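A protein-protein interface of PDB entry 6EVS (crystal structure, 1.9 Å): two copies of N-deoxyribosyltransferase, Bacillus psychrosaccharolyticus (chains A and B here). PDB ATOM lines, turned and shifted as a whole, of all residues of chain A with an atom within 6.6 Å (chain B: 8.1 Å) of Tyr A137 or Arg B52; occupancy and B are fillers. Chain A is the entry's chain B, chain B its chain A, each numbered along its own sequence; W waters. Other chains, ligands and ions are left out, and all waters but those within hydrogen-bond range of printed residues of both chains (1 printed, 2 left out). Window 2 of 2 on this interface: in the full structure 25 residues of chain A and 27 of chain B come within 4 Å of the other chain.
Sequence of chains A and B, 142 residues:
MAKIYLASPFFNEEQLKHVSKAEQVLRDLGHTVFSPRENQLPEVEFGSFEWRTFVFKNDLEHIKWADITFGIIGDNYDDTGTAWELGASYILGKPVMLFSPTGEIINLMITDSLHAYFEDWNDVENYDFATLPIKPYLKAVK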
ATOM      1  N   LEU A  98      16.629  30.534  26.580  1.00  0.00           N
ATOM      2  CA  LEU A  98      17.595  30.364  27.649  1.00  0.00           C
ATOM      3  C   LEU A  98      18.779  31.284  27.406  1.00  0.00           C
ATOM      4  O   LEU A  98      19.332  31.324  26.303  1.00  0.00           O
ATOM      5  CB  LEU A  98      18.051  28.899  27.771  1.00  0.00           C
ATOM      6  CG  LEU A  98      18.998  28.600  28.947  1.00  0.00           C
ATOM      7  CD1 LEU A  98      18.266  28.595  30.292  1.00  0.00           C
ATOM      8  CD2 LEU A  98      19.738  27.291  28.742  1.00  0.00           C
ATOM      9  N   GLY A 103      28.113  30.035  29.559  1.00  0.00           N
ATOM     10  CA  GLY A 103      28.326  29.411  28.263  1.00  0.00           C
ATOM     11  C   GLY A 103      28.828  27.987  28.353  1.00  0.00           C
ATOM     12  O   GLY A 103      29.596  27.548  27.492  1.00  0.00           O
ATOM     13  N   GLU A 104      28.408  27.245  29.378  1.00  0.00           N
ATOM     14  CA  GLU A 104      28.934  25.912  29.651  1.00  0.00           C
ATOM     15  C   GLU A 104      28.153  24.854  28.879  1.00  0.00           C
ATOM     16  O   GLU A 104      27.754  25.082  27.730  1.00  0.00           O
ATOM     17  CB  GLU A 104      28.890  25.658  31.160  1.00  0.00           C
ATOM     18  CG  GLU A 104      29.516  24.368  31.690  1.00  0.00           C
ATOM     19  CD  GLU A 104      30.154  24.594  33.001  1.00  0.00           C
ATOM     20  OE1 GLU A 104      31.162  23.929  33.321  1.00  0.00           O
ATOM     21  OE2 GLU A 104      29.688  25.519  33.680  1.00  0.00           O
ATOM     22  N   ILE A 105      27.942  23.697  29.500  1.00  0.00           N
ATOM     23  CA  ILE A 105      27.206  22.581  28.933  1.00  0.00           C
ATOM     24  C   ILE A 105      26.000  22.351  29.829  1.00  0.00           C
ATOM     25  O   ILE A 105      26.148  22.101  31.032  1.00  0.00           O
ATOM     26  CB  ILE A 105      28.067  21.311  28.830  1.00  0.00           C
ATOM     27  CG1 ILE A 105      29.290  21.554  27.937  1.00  0.00           C
ATOM     28  CG2 ILE A 105      27.238  20.144  28.307  1.00  0.00           C
ATOM     29  CD1 ILE A 105      30.535  21.964  28.691  1.00  0.00           C
ATOM     30  N   ILE A 106      24.817  22.455  29.258  1.00  0.00           N
ATOM     31  CA  ILE A 106      23.582  22.300  30.012  1.00  0.00           C
ATOM     32  C   ILE A 106      22.965  20.951  29.658  1.00  0.00           C
ATOM     33  O   ILE A 106      23.205  20.396  28.580  1.00  0.00           O
ATOM     34  CB  ILE A 106      22.627  23.484  29.735  1.00  0.00           C
ATOM     35  CG1 ILE A 106      23.250  24.778  30.267  1.00  0.00           C
ATOM     36  CG2 ILE A 106      21.253  23.273  30.362  1.00  0.00           C
ATOM     37  CD1 ILE A 106      23.125  25.948  29.321  1.00  0.00           C
ATOM     38  N   ASN A 107      22.200  20.411  30.606  1.00  0.00           N
ATOM     39  CA  ASN A 107      21.586  19.098  30.488  1.00  0.00           C
ATOM     40  C   ASN A 107      20.827  18.961  29.164  1.00  0.00           C
ATOM     41  O   ASN A 107      20.274  19.929  28.642  1.00  0.00           O
ATOM     42  CB  ASN A 107      20.656  18.891  31.693  1.00  0.00           C
ATOM     43  CG  ASN A 107      19.918  17.569  31.655  1.00  0.00           C
ATOM     44  OD1 ASN A 107      18.854  17.457  31.054  1.00  0.00           O
ATOM     45  ND2 ASN A 107      20.475  16.564  32.317  1.00  0.00           N
ATOM     46  N   LEU A 108      20.837  17.743  28.616  1.00  0.00           N
ATOM     47  CA  LEU A 108      20.179  17.420  27.348  1.00  0.00           C
ATOM     48  C   LEU A 108      18.703  17.853  27.326  1.00  0.00           C
ATOM     49  O   LEU A 108      18.225  18.439  26.340  1.00  0.00           O
ATOM     50  CB  LEU A 108      20.318  15.912  27.121  1.00  0.00           C
ATOM     51  CG  LEU A 108      19.789  15.136  25.909  1.00  0.00           C
ATOM     52  CD1 LEU A 108      20.868  14.184  25.444  1.00  0.00           C
ATOM     53  CD2 LEU A 108      18.537  14.364  26.287  1.00  0.00           C
ATOM     54  N   THR A 111      18.466  21.768  26.829  1.00  0.00           N
ATOM     55  CA  THR A 111      18.934  22.292  25.548  1.00  0.00           C
ATOM     56  C   THR A 111      18.067  21.807  24.388  1.00  0.00           C
ATOM     57  O   THR A 111      17.754  22.579  23.474  1.00  0.00           O
ATOM     58  CB  THR A 111      20.404  21.913  25.336  1.00  0.00           C
ATOM     59  OG1 THR A 111      20.522  20.496  25.133  1.00  0.00           O
ATOM     60  CG2 THR A 111      21.212  22.306  26.550  1.00  0.00           C
ATOM     61  N   ASP A 112      17.655  20.537  24.411  1.00  0.00           N
ATOM     62  CA  ASP A 112      16.820  20.026  23.331  1.00  0.00           C
ATOM     63  C   ASP A 112      15.429  20.637  23.333  1.00  0.00           C
ATOM     64  O   ASP A 112      14.749  20.602  22.307  1.00  0.00           O
ATOM     65  CB  ASP A 112      16.715  18.504  23.398  1.00  0.00           C
ATOM     66  CG  ASP A 112      17.564  17.834  22.332  1.00  0.00           C
ATOM     67  OD1 ASP A 112      18.386  18.553  21.743  1.00  0.00           O
ATOM     68  OD2 ASP A 112      17.408  16.625  22.059  1.00  0.00           O
ATOM     69  N   LEU A 114      14.756  23.921  24.134  1.00  0.00           N
ATOM     70  CA  LEU A 114      14.770  25.356  23.909  1.00  0.00           C
ATOM     71  C   LEU A 114      14.371  25.680  22.481  1.00  0.00           C
ATOM     72  O   LEU A 114      14.628  24.912  21.549  1.00  0.00           O
ATOM     73  CB  LEU A 114      16.165  25.933  24.174  1.00  0.00           C
ATOM     74  CG  LEU A 114      16.817  25.602  25.507  1.00  0.00           C
ATOM     75  CD1 LEU A 114      18.285  26.053  25.522  1.00  0.00           C
ATOM     76  CD2 LEU A 114      16.017  26.227  26.647  1.00  0.00           C
ATOM     77  N   HIS A 115      13.756  26.847  22.313  1.00  0.00           N
ATOM     78  CA  HIS A 115      13.562  27.424  20.984  1.00  0.00           C
ATOM     79  C   HIS A 115      14.642  28.426  20.619  1.00  0.00           C
ATOM     80  O   HIS A 115      15.001  28.534  19.446  1.00  0.00           O
ATOM     81  CB  HIS A 115      12.195  28.121  20.885  1.00  0.00           C
ATOM     82  CG  HIS A 115      11.856  28.597  19.501  1.00  0.00           C
ATOM     83  ND1 HIS A 115      11.492  27.737  18.489  1.00  0.00           N
ATOM     84  CD2 HIS A 115      11.859  29.838  18.954  1.00  0.00           C
ATOM     85  CE1 HIS A 115      11.278  28.425  17.378  1.00  0.00           C
ATOM     86  NE2 HIS A 115      11.493  29.705  17.634  1.00  0.00           N
ATOM     87  N   ALA A 116      15.173  29.166  21.592  1.00  0.00           N
ATOM     88  CA  ALA A 116      16.204  30.149  21.318  1.00  0.00           C
ATOM     89  C   ALA A 116      17.188  30.154  22.478  1.00  0.00           C
ATOM     90  O   ALA A 116      16.785  30.113  23.644  1.00  0.00           O
ATOM     91  CB  ALA A 116      15.611  31.546  21.095  1.00  0.00           C
ATOM     92  N   TYR A 117      18.471  30.164  22.142  1.00  0.00           N
ATOM     93  CA  TYR A 117      19.555  30.116  23.112  1.00  0.00           C
ATOM     94  C   TYR A 117      20.472  31.316  22.901  1.00  0.00           C
ATOM     95  O   TYR A 117      20.840  31.632  21.765  1.00  0.00           O
ATOM     96  CB  TYR A 117      20.339  28.801  22.977  1.00  0.00           C
ATOM     97  CG  TYR A 117      21.583  28.750  23.835  1.00  0.00           C
ATOM     98  CD1 TYR A 117      21.489  28.600  25.207  1.00  0.00           C
ATOM     99  CD2 TYR A 117      22.851  28.851  23.270  1.00  0.00           C
ATOM    100  CE1 TYR A 117      22.630  28.564  26.011  1.00  0.00           C
ATOM    101  CE2 TYR A 117      24.005  28.807  24.063  1.00  0.00           C
ATOM    102  CZ  TYR A 117      23.882  28.655  25.432  1.00  0.00           C
ATOM    103  OH  TYR A 117      24.993  28.615  26.245  1.00  0.00           O
ATOM    104  N   GLU A 119      23.917  33.766  24.542  1.00  0.00           N
ATOM    105  CA  GLU A 119      25.030  33.932  25.462  1.00  0.00           C
ATOM    106  C   GLU A 119      25.485  35.378  25.574  1.00  0.00           C
ATOM    107  O   GLU A 119      26.460  35.646  26.285  1.00  0.00           O
ATOM    108  CB  GLU A 119      26.224  33.050  25.043  1.00  0.00           C
ATOM    109  CG  GLU A 119      26.087  31.575  25.440  1.00  0.00           C
ATOM    110  CD  GLU A 119      27.243  30.718  24.942  1.00  0.00           C
ATOM    111  OE1 GLU A 119      28.297  31.289  24.601  1.00  0.00           O
ATOM    112  OE2 GLU A 119      27.112  29.475  24.910  1.00  0.00           O
ATOM    113  N   LYS A 135      16.661  29.376  17.179  1.00  0.00           N
ATOM    114  CA  LYS A 135      18.098  29.564  17.391  1.00  0.00           C
ATOM    115  C   LYS A 135      18.591  28.492  18.333  1.00  0.00           C
ATOM    116  O   LYS A 135      18.707  28.695  19.554  1.00  0.00           O
ATOM    117  CB  LYS A 135      18.385  30.969  17.939  1.00  0.00           C
ATOM    118  CG  LYS A 135      17.714  32.021  17.133  1.00  0.00           C
ATOM    119  CD  LYS A 135      18.740  32.871  16.518  1.00  0.00           C
ATOM    120  CE  LYS A 135      18.168  33.826  15.577  1.00  0.00           C
ATOM    121  NZ  LYS A 135      19.161  34.885  15.416  1.00  0.00           N
ATOM    122  N   PRO A 136      18.875  27.324  17.801  1.00  0.00           N
ATOM    123  CA  PRO A 136      19.030  26.149  18.650  1.00  0.00           C
ATOM    124  C   PRO A 136      20.402  26.110  19.308  1.00  0.00           C
ATOM    125  O   PRO A 136      21.351  26.771  18.885  1.00  0.00           O
ATOM    126  CB  PRO A 136      18.851  24.972  17.672  1.00  0.00           C
ATOM    127  CG  PRO A 136      18.936  25.574  16.281  1.00  0.00           C
ATOM    128  CD  PRO A 136      19.188  27.038  16.384  1.00  0.00           C
ATOM    129  N   TYR A 137      20.466  25.358  20.397  1.00  0.00           N
ATOM    130  CA  TYR A 137      21.725  25.087  21.065  1.00  0.00           C
ATOM    131  C   TYR A 137      22.473  24.027  20.274  1.00  0.00           C
ATOM    132  O   TYR A 137      21.939  22.939  20.033  1.00  0.00           O
ATOM    133  CB  TYR A 137      21.457  24.621  22.493  1.00  0.00           C
ATOM    134  CG  TYR A 137      22.667  24.173  23.283  1.00  0.00           C
ATOM    135  CD1 TYR A 137      23.355  25.068  24.090  1.00  0.00           C
ATOM    136  CD2 TYR A 137      23.094  22.848  23.259  1.00  0.00           C
ATOM    137  CE1 TYR A 137      24.446  24.664  24.830  1.00  0.00           C
ATOM    138  CE2 TYR A 137      24.179  22.438  24.000  1.00  0.00           C
ATOM    139  CZ  TYR A 137      24.848  23.353  24.782  1.00  0.00           C
ATOM    140  OH  TYR A 137      25.923  22.967  25.530  1.00  0.00           O
ATOM    141  N   LEU A 138      23.699  24.343  19.868  1.00  0.00           N
ATOM    142  CA  LEU A 138      24.521  23.407  19.109  1.00  0.00           C
ATOM    143  C   LEU A 138      26.016  23.646  19.319  1.00  0.00           C
ATOM    144  O   LEU A 138      26.697  22.859  19.980  1.00  0.00           O
ATOM    145  CB  LEU A 138      24.186  23.499  17.624  1.00  0.00           C
ATOM    146  CG  LEU A 138      23.399  22.307  17.080  1.00  0.00           C
ATOM    147  CD1 LEU A 138      22.875  22.623  15.692  1.00  0.00           C
ATOM    148  CD2 LEU A 138      24.280  21.056  17.065  1.00  0.00           C
ATOM    149  N   LEU B  41      20.948   3.811  24.517  1.00  0.00           N
ATOM    150  CA  LEU B  41      20.789   3.479  23.101  1.00  0.00           C
ATOM    151  C   LEU B  41      22.026   2.772  22.562  1.00  0.00           C
ATOM    152  O   LEU B  41      23.126   3.327  22.623  1.00  0.00           O
ATOM    153  CB  LEU B  41      20.450   4.743  22.306  1.00  0.00           C
ATOM    154  CG  LEU B  41      19.086   5.267  22.786  1.00  0.00           C
ATOM    155  CD1 LEU B  41      18.571   6.431  21.943  1.00  0.00           C
ATOM    156  CD2 LEU B  41      18.070   4.132  22.796  1.00  0.00           C
ATOM    157  N   VAL B  44      23.800   4.182  18.621  1.00  0.00           N
ATOM    158  CA  VAL B  44      24.053   5.427  17.920  1.00  0.00           C
ATOM    159  C   VAL B  44      25.258   6.093  18.567  1.00  0.00           C
ATOM    160  O   VAL B  44      25.438   6.021  19.788  1.00  0.00           O
ATOM    161  CB  VAL B  44      22.801   6.322  17.986  1.00  0.00           C
ATOM    162  CG1 VAL B  44      23.154   7.770  17.733  1.00  0.00           C
ATOM    163  CG2 VAL B  44      21.759   5.846  16.999  1.00  0.00           C
ATOM    164  N   GLU B  45      26.106   6.726  17.752  1.00  0.00           N
ATOM    165  CA  GLU B  45      27.309   7.364  18.277  1.00  0.00           C
ATOM    166  C   GLU B  45      26.968   8.270  19.449  1.00  0.00           C
ATOM    167  O   GLU B  45      26.066   9.110  19.357  1.00  0.00           O
ATOM    168  CB  GLU B  45      28.020   8.167  17.187  1.00  0.00           C
ATOM    169  CG  GLU B  45      29.192   8.990  17.719  1.00  0.00           C
ATOM    170  CD  GLU B  45      30.099   9.496  16.625  1.00  0.00           C
ATOM    171  OE1 GLU B  45      31.333   9.315  16.737  1.00  0.00           O
ATOM    172  OE2 GLU B  45      29.577  10.076  15.649  1.00  0.00           O
ATOM    173  N   PHE B  46      27.672   8.069  20.562  1.00  0.00           N
ATOM    174  CA  PHE B  46      27.402   8.857  21.756  1.00  0.00           C
ATOM    175  C   PHE B  46      27.617  10.336  21.465  1.00  0.00           C
ATOM    176  O   PHE B  46      28.554  10.716  20.759  1.00  0.00           O
ATOM    177  CB  PHE B  46      28.289   8.401  22.922  1.00  0.00           C
ATOM    178  CG  PHE B  46      27.544   8.265  24.225  1.00  0.00           C
ATOM    179  CD1 PHE B  46      26.660   7.211  24.427  1.00  0.00           C
ATOM    180  CD2 PHE B  46      27.702   9.202  25.236  1.00  0.00           C
ATOM    181  CE1 PHE B  46      25.955   7.082  25.617  1.00  0.00           C
ATOM    182  CE2 PHE B  46      27.004   9.082  26.427  1.00  0.00           C
ATOM    183  CZ  PHE B  46      26.127   8.018  26.621  1.00  0.00           C
ATOM    184  N   GLY B  47      26.707  11.171  21.965  1.00  0.00           N
ATOM    185  CA  GLY B  47      26.848  12.605  21.841  1.00  0.00           C
ATOM    186  C   GLY B  47      26.579  13.180  20.469  1.00  0.00           C
ATOM    187  O   GLY B  47      26.610  14.408  20.317  1.00  0.00           O
ATOM    188  N   SER B  48      26.328  12.348  19.464  1.00  0.00           N
ATOM    189  CA  SER B  48      25.934  12.864  18.163  1.00  0.00           C
ATOM    190  C   SER B  48      24.576  13.570  18.253  1.00  0.00           C
ATOM    191  O   SER B  48      23.828  13.429  19.233  1.00  0.00           O
ATOM    192  CB  SER B  48      25.870  11.729  17.145  1.00  0.00           C
ATOM    193  OG  SER B  48      24.838  10.821  17.510  1.00  0.00           O
ATOM    194  N   PHE B  49      24.258  14.346  17.211  1.00  0.00           N
ATOM    195  CA  PHE B  49      22.921  14.936  17.129  1.00  0.00           C
ATOM    196  C   PHE B  49      21.846  13.857  17.096  1.00  0.00           C
ATOM    197  O   PHE B  49      20.800  13.994  17.744  1.00  0.00           O
ATOM    198  CB  PHE B  49      22.792  15.841  15.900  1.00  0.00           C
ATOM    199  CG  PHE B  49      21.490  16.589  15.856  1.00  0.00           C
ATOM    200  CD1 PHE B  49      21.326  17.743  16.598  1.00  0.00           C
ATOM    201  CD2 PHE B  49      20.425  16.120  15.113  1.00  0.00           C
ATOM    202  CE1 PHE B  49      20.129  18.425  16.594  1.00  0.00           C
ATOM    203  CE2 PHE B  49      19.221  16.800  15.108  1.00  0.00           C
ATOM    204  CZ  PHE B  49      19.079  17.956  15.851  1.00  0.00           C
ATOM    205  N   GLU B  50      22.073  12.785  16.330  1.00  0.00           N
ATOM    206  CA  GLU B  50      21.135  11.664  16.336  1.00  0.00           C
ATOM    207  C   GLU B  50      20.923  11.116  17.748  1.00  0.00           C
ATOM    208  O   GLU B  50      19.789  10.837  18.159  1.00  0.00           O
ATOM    209  CB  GLU B  50      21.646  10.561  15.407  1.00  0.00           C
ATOM    210  CG  GLU B  50      20.680   9.406  15.213  1.00  0.00           C
ATOM    211  CD  GLU B  50      21.061   8.509  14.063  1.00  0.00           C
ATOM    212  OE1 GLU B  50      21.438   7.334  14.302  1.00  0.00           O
ATOM    213  OE2 GLU B  50      20.995   8.964  12.898  1.00  0.00           O
ATOM    214  N   TRP B  51      22.017  10.937  18.501  1.00  0.00           N
ATOM    215  CA  TRP B  51      21.915  10.374  19.845  1.00  0.00           C
ATOM    216  C   TRP B  51      21.183  11.323  20.789  1.00  0.00           C
ATOM    217  O   TRP B  51      20.290  10.897  21.539  1.00  0.00           O
ATOM    218  CB  TRP B  51      23.323  10.026  20.371  1.00  0.00           C
ATOM    219  CG  TRP B  51      23.295   9.549  21.782  1.00  0.00           C
ATOM    220  CD1 TRP B  51      23.142   8.263  22.218  1.00  0.00           C
ATOM    221  CD2 TRP B  51      23.388  10.362  22.951  1.00  0.00           C
ATOM    222  NE1 TRP B  51      23.130   8.229  23.594  1.00  0.00           N
ATOM    223  CE2 TRP B  51      23.288   9.505  24.068  1.00  0.00           C
ATOM    224  CE3 TRP B  51      23.560  11.735  23.165  1.00  0.00           C
ATOM    225  CZ2 TRP B  51      23.344   9.979  25.379  1.00  0.00           C
ATOM    226  CZ3 TRP B  51      23.620  12.202  24.471  1.00  0.00           C
ATOM    227  CH2 TRP B  51      23.499  11.327  25.556  1.00  0.00           C
ATOM    228  N   ARG B  52      21.514  12.618  20.743  1.00  0.00           N
ATOM    229  CA  ARG B  52      20.822  13.589  21.589  1.00  0.00           C
ATOM    230  C   ARG B  52      19.323  13.631  21.269  1.00  0.00           C
ATOM    231  O   ARG B  52      18.484  13.715  22.173  1.00  0.00           O
ATOM    232  CB  ARG B  52      21.467  14.975  21.430  1.00  0.00           C
ATOM    233  CG  ARG B  52      20.662  15.959  20.596  1.00  0.00           C
ATOM    234  CD  ARG B  52      21.295  17.336  20.429  1.00  0.00           C
ATOM    235  NE  ARG B  52      20.290  18.324  20.020  1.00  0.00           N
ATOM    236  CZ  ARG B  52      20.506  19.636  19.981  1.00  0.00           C
ATOM    237  NH1 ARG B  52      21.694  20.116  20.339  1.00  0.00           N
ATOM    238  NH2 ARG B  52      19.536  20.470  19.606  1.00  0.00           N
ATOM    239  N   THR B  53      18.970  13.540  19.990  1.00  0.00           N
ATOM    240  CA  THR B  53      17.566  13.596  19.591  1.00  0.00           C
ATOM    241  C   THR B  53      16.816  12.363  20.065  1.00  0.00           C
ATOM    242  O   THR B  53      15.731  12.477  20.651  1.00  0.00           O
ATOM    243  CB  THR B  53      17.469  13.746  18.075  1.00  0.00           C
ATOM    244  OG1 THR B  53      18.241  14.876  17.667  1.00  0.00           O
ATOM    245  CG2 THR B  53      15.993  13.898  17.624  1.00  0.00           C
ATOM    246  N   PHE B  54      17.366  11.171  19.798  1.00  0.00           N
ATOM    247  CA  PHE B  54      16.645   9.949  20.140  1.00  0.00           C
ATOM    248  C   PHE B  54      16.487   9.796  21.648  1.00  0.00           C
ATOM    249  O   PHE B  54      15.440   9.344  22.123  1.00  0.00           O
ATOM    250  CB  PHE B  54      17.354   8.736  19.550  1.00  0.00           C
ATOM    251  CG  PHE B  54      17.150   8.584  18.070  1.00  0.00           C
ATOM    252  CD1 PHE B  54      16.074   9.193  17.439  1.00  0.00           C
ATOM    253  CD2 PHE B  54      18.041   7.846  17.307  1.00  0.00           C
ATOM    254  CE1 PHE B  54      15.881   9.061  16.057  1.00  0.00           C
ATOM    255  CE2 PHE B  54      17.849   7.707  15.936  1.00  0.00           C
ATOM    256  CZ  PHE B  54      16.766   8.318  15.315  1.00  0.00           C
ATOM    257  N   VAL B  55      17.518  10.150  22.412  1.00  0.00           N
ATOM    258  CA  VAL B  55      17.419  10.022  23.863  1.00  0.00           C
ATOM    259  C   VAL B  55      16.338  10.948  24.400  1.00  0.00           C
ATOM    260  O   VAL B  55      15.481  10.539  25.196  1.00  0.00           O
ATOM    261  CB  VAL B  55      18.782  10.295  24.520  1.00  0.00           C
ATOM    262  CG1 VAL B  55      18.592  10.544  26.022  1.00  0.00           C
ATOM    263  CG2 VAL B  55      19.740   9.129  24.279  1.00  0.00           C
ATOM    264  N   PHE B  56      16.370  12.217  23.990  1.00  0.00           N
ATOM    265  CA  PHE B  56      15.323  13.149  24.393  1.00  0.00           C
ATOM    266  C   PHE B  56      13.944  12.615  24.025  1.00  0.00           C
ATOM    267  O   PHE B  56      13.047  12.534  24.870  1.00  0.00           O
ATOM    268  CB  PHE B  56      15.560  14.511  23.739  1.00  0.00           C
ATOM    269  CG  PHE B  56      14.545  15.548  24.133  1.00  0.00           C
ATOM    270  CD1 PHE B  56      14.707  16.304  25.295  1.00  0.00           C
ATOM    271  CD2 PHE B  56      13.446  15.761  23.353  1.00  0.00           C
ATOM    272  CE1 PHE B  56      13.757  17.272  25.657  1.00  0.00           C
ATOM    273  CE2 PHE B  56      12.468  16.719  23.713  1.00  0.00           C
ATOM    274  CZ  PHE B  56      12.635  17.466  24.878  1.00  0.00           C
ATOM    275  N   LYS B  57      13.775  12.215  22.762  1.00  0.00           N
ATOM    276  CA  LYS B  57      12.464  11.776  22.296  1.00  0.00           C
ATOM    277  C   LYS B  57      12.033  10.506  23.006  1.00  0.00           C
ATOM    278  O   LYS B  57      10.880  10.385  23.417  1.00  0.00           O
ATOM    279  CB  LYS B  57      12.483  11.561  20.781  1.00  0.00           C
ATOM    280  CG  LYS B  57      12.533  12.846  19.994  1.00  0.00           C
ATOM    281  CD  LYS B  57      12.557  12.568  18.477  1.00  0.00           C
ATOM    282  CE  LYS B  57      12.451  13.863  17.685  1.00  0.00           C
ATOM    283  NZ  LYS B  57      11.778  13.692  16.360  1.00  0.00           N
ATOM    284  N   ASN B  58      12.961   9.562  23.203  1.00  0.00           N
ATOM    285  CA  ASN B  58      12.575   8.318  23.855  1.00  0.00           C
ATOM    286  C   ASN B  58      12.222   8.559  25.312  1.00  0.00           C
ATOM    287  O   ASN B  58      11.275   7.959  25.839  1.00  0.00           O
ATOM    288  CB  ASN B  58      13.702   7.288  23.745  1.00  0.00           C
ATOM    289  CG  ASN B  58      13.242   5.888  24.103  1.00  0.00           C
ATOM    290  OD1 ASN B  58      12.105   5.502  23.804  1.00  0.00           O
ATOM    291  ND2 ASN B  58      14.113   5.122  24.747  1.00  0.00           N
ATOM    292  N   ASP B  59      12.978   9.434  25.978  1.00  0.00           N
ATOM    293  CA  ASP B  59      12.721   9.737  27.387  1.00  0.00           C
ATOM    294  C   ASP B  59      11.354  10.383  27.554  1.00  0.00           C
ATOM    295  O   ASP B  59      10.530   9.933  28.363  1.00  0.00           O
ATOM    296  CB  ASP B  59      13.817  10.658  27.936  1.00  0.00           C
ATOM    297  CG  ASP B  59      15.123   9.920  28.244  1.00  0.00           C
ATOM    298  OD1 ASP B  59      15.189   8.687  28.028  1.00  0.00           O
ATOM    299  OD2 ASP B  59      16.073  10.582  28.700  1.00  0.00           O
HETATM  300  O   HOH W   1      18.200  17.238  19.226  1.00  0.00           O
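Water W1 lies within hydrogen-bond range of the guanidinium group (NE) of Arg B52, the side-chain hydroxyl (OG1) of Thr B53 and the side-chain carboxylate (OD1) of Asp A112.
No position is printed for both chains. Of the 8 pairs that touch across the chains among the printed residues, none has its exchanged pair printed and touching as well.
The backbone NH of Trp B51 is in hydrogen-bond range of the side-chain hydroxyl of Ser B48. The backbone carbonyl oxygen (O) of Leu A108 lies within hydrogen-bond range of the side-chain hydroxyl (OG1) of Thr A111 (3.3 Å). The side-chain hydroxyl (OG1) of Thr B53 sits at hydrogen-bond distance from the backbone carbonyl oxygen (O) of Phe B49, at 2.7 Å.
Among the printed residues, merely in contact across the chains: Leu A108 with Trp B51 (3.5 Å), Leu A108 with Arg B52 (3.9 Å), Leu A108 with Val B55 (3.8 Å), Leu A108 with Phe B56 (3.8 Å), Asp A112 with Thr B53 (3.9 Å) and Asp A112 with Phe B56 (3.3 Å).
NH1 of Arg B52 is in hydrogen-bond range of O of Tyr A137, at 2.9 Å. The guanidinium group of Arg B52 lies within salt-bridge range of the side-chain carboxylate of Asp A112.
Of chain B, only Arg B52 comes within 4 Å of Tyr A137. Of chain A, only Leu A108 (3.9 Å), Asp A112 (2.6 Å) and Tyr A137 (2.9 Å) come within 4 Å of Arg B52. Printed residues of chain B within 4 Å of Asp A112: Arg B52 (2.6 Å), Thr B53 (3.9 Å) and Phe B56 (3.3 Å). Of the printed residues of chain B, Leu A108 touches Trp B51 (3.5 Å), Arg B52 (3.9 Å), Val B55 (3.8 Å) and Phe B56 (3.8 Å). Of the printed residues of chain A, Val B55 touches Leu A108 (3.8 Å). Printed residues of chain A within 4 Å of Trp B51: Leu A108 (3.5 Å). Of the printed residues of chain A, Phe B56 touches Leu A108 and Asp A112. The nearest residue of chain B that does not touch Tyr A137 is Phe B49 (6.0 Å). The nearest printed residue of chain A that does not touch Phe B56 is Thr A111 (6.4 Å).
Hydrophobic or aromatic side chains of chain A within 4 Å of the printed part of chain B: Leu A108. Hydrophobic or aromatic side chains of chain B within 4 Å of the printed part of chain A: Trp B51, Val B55 and Phe B56.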
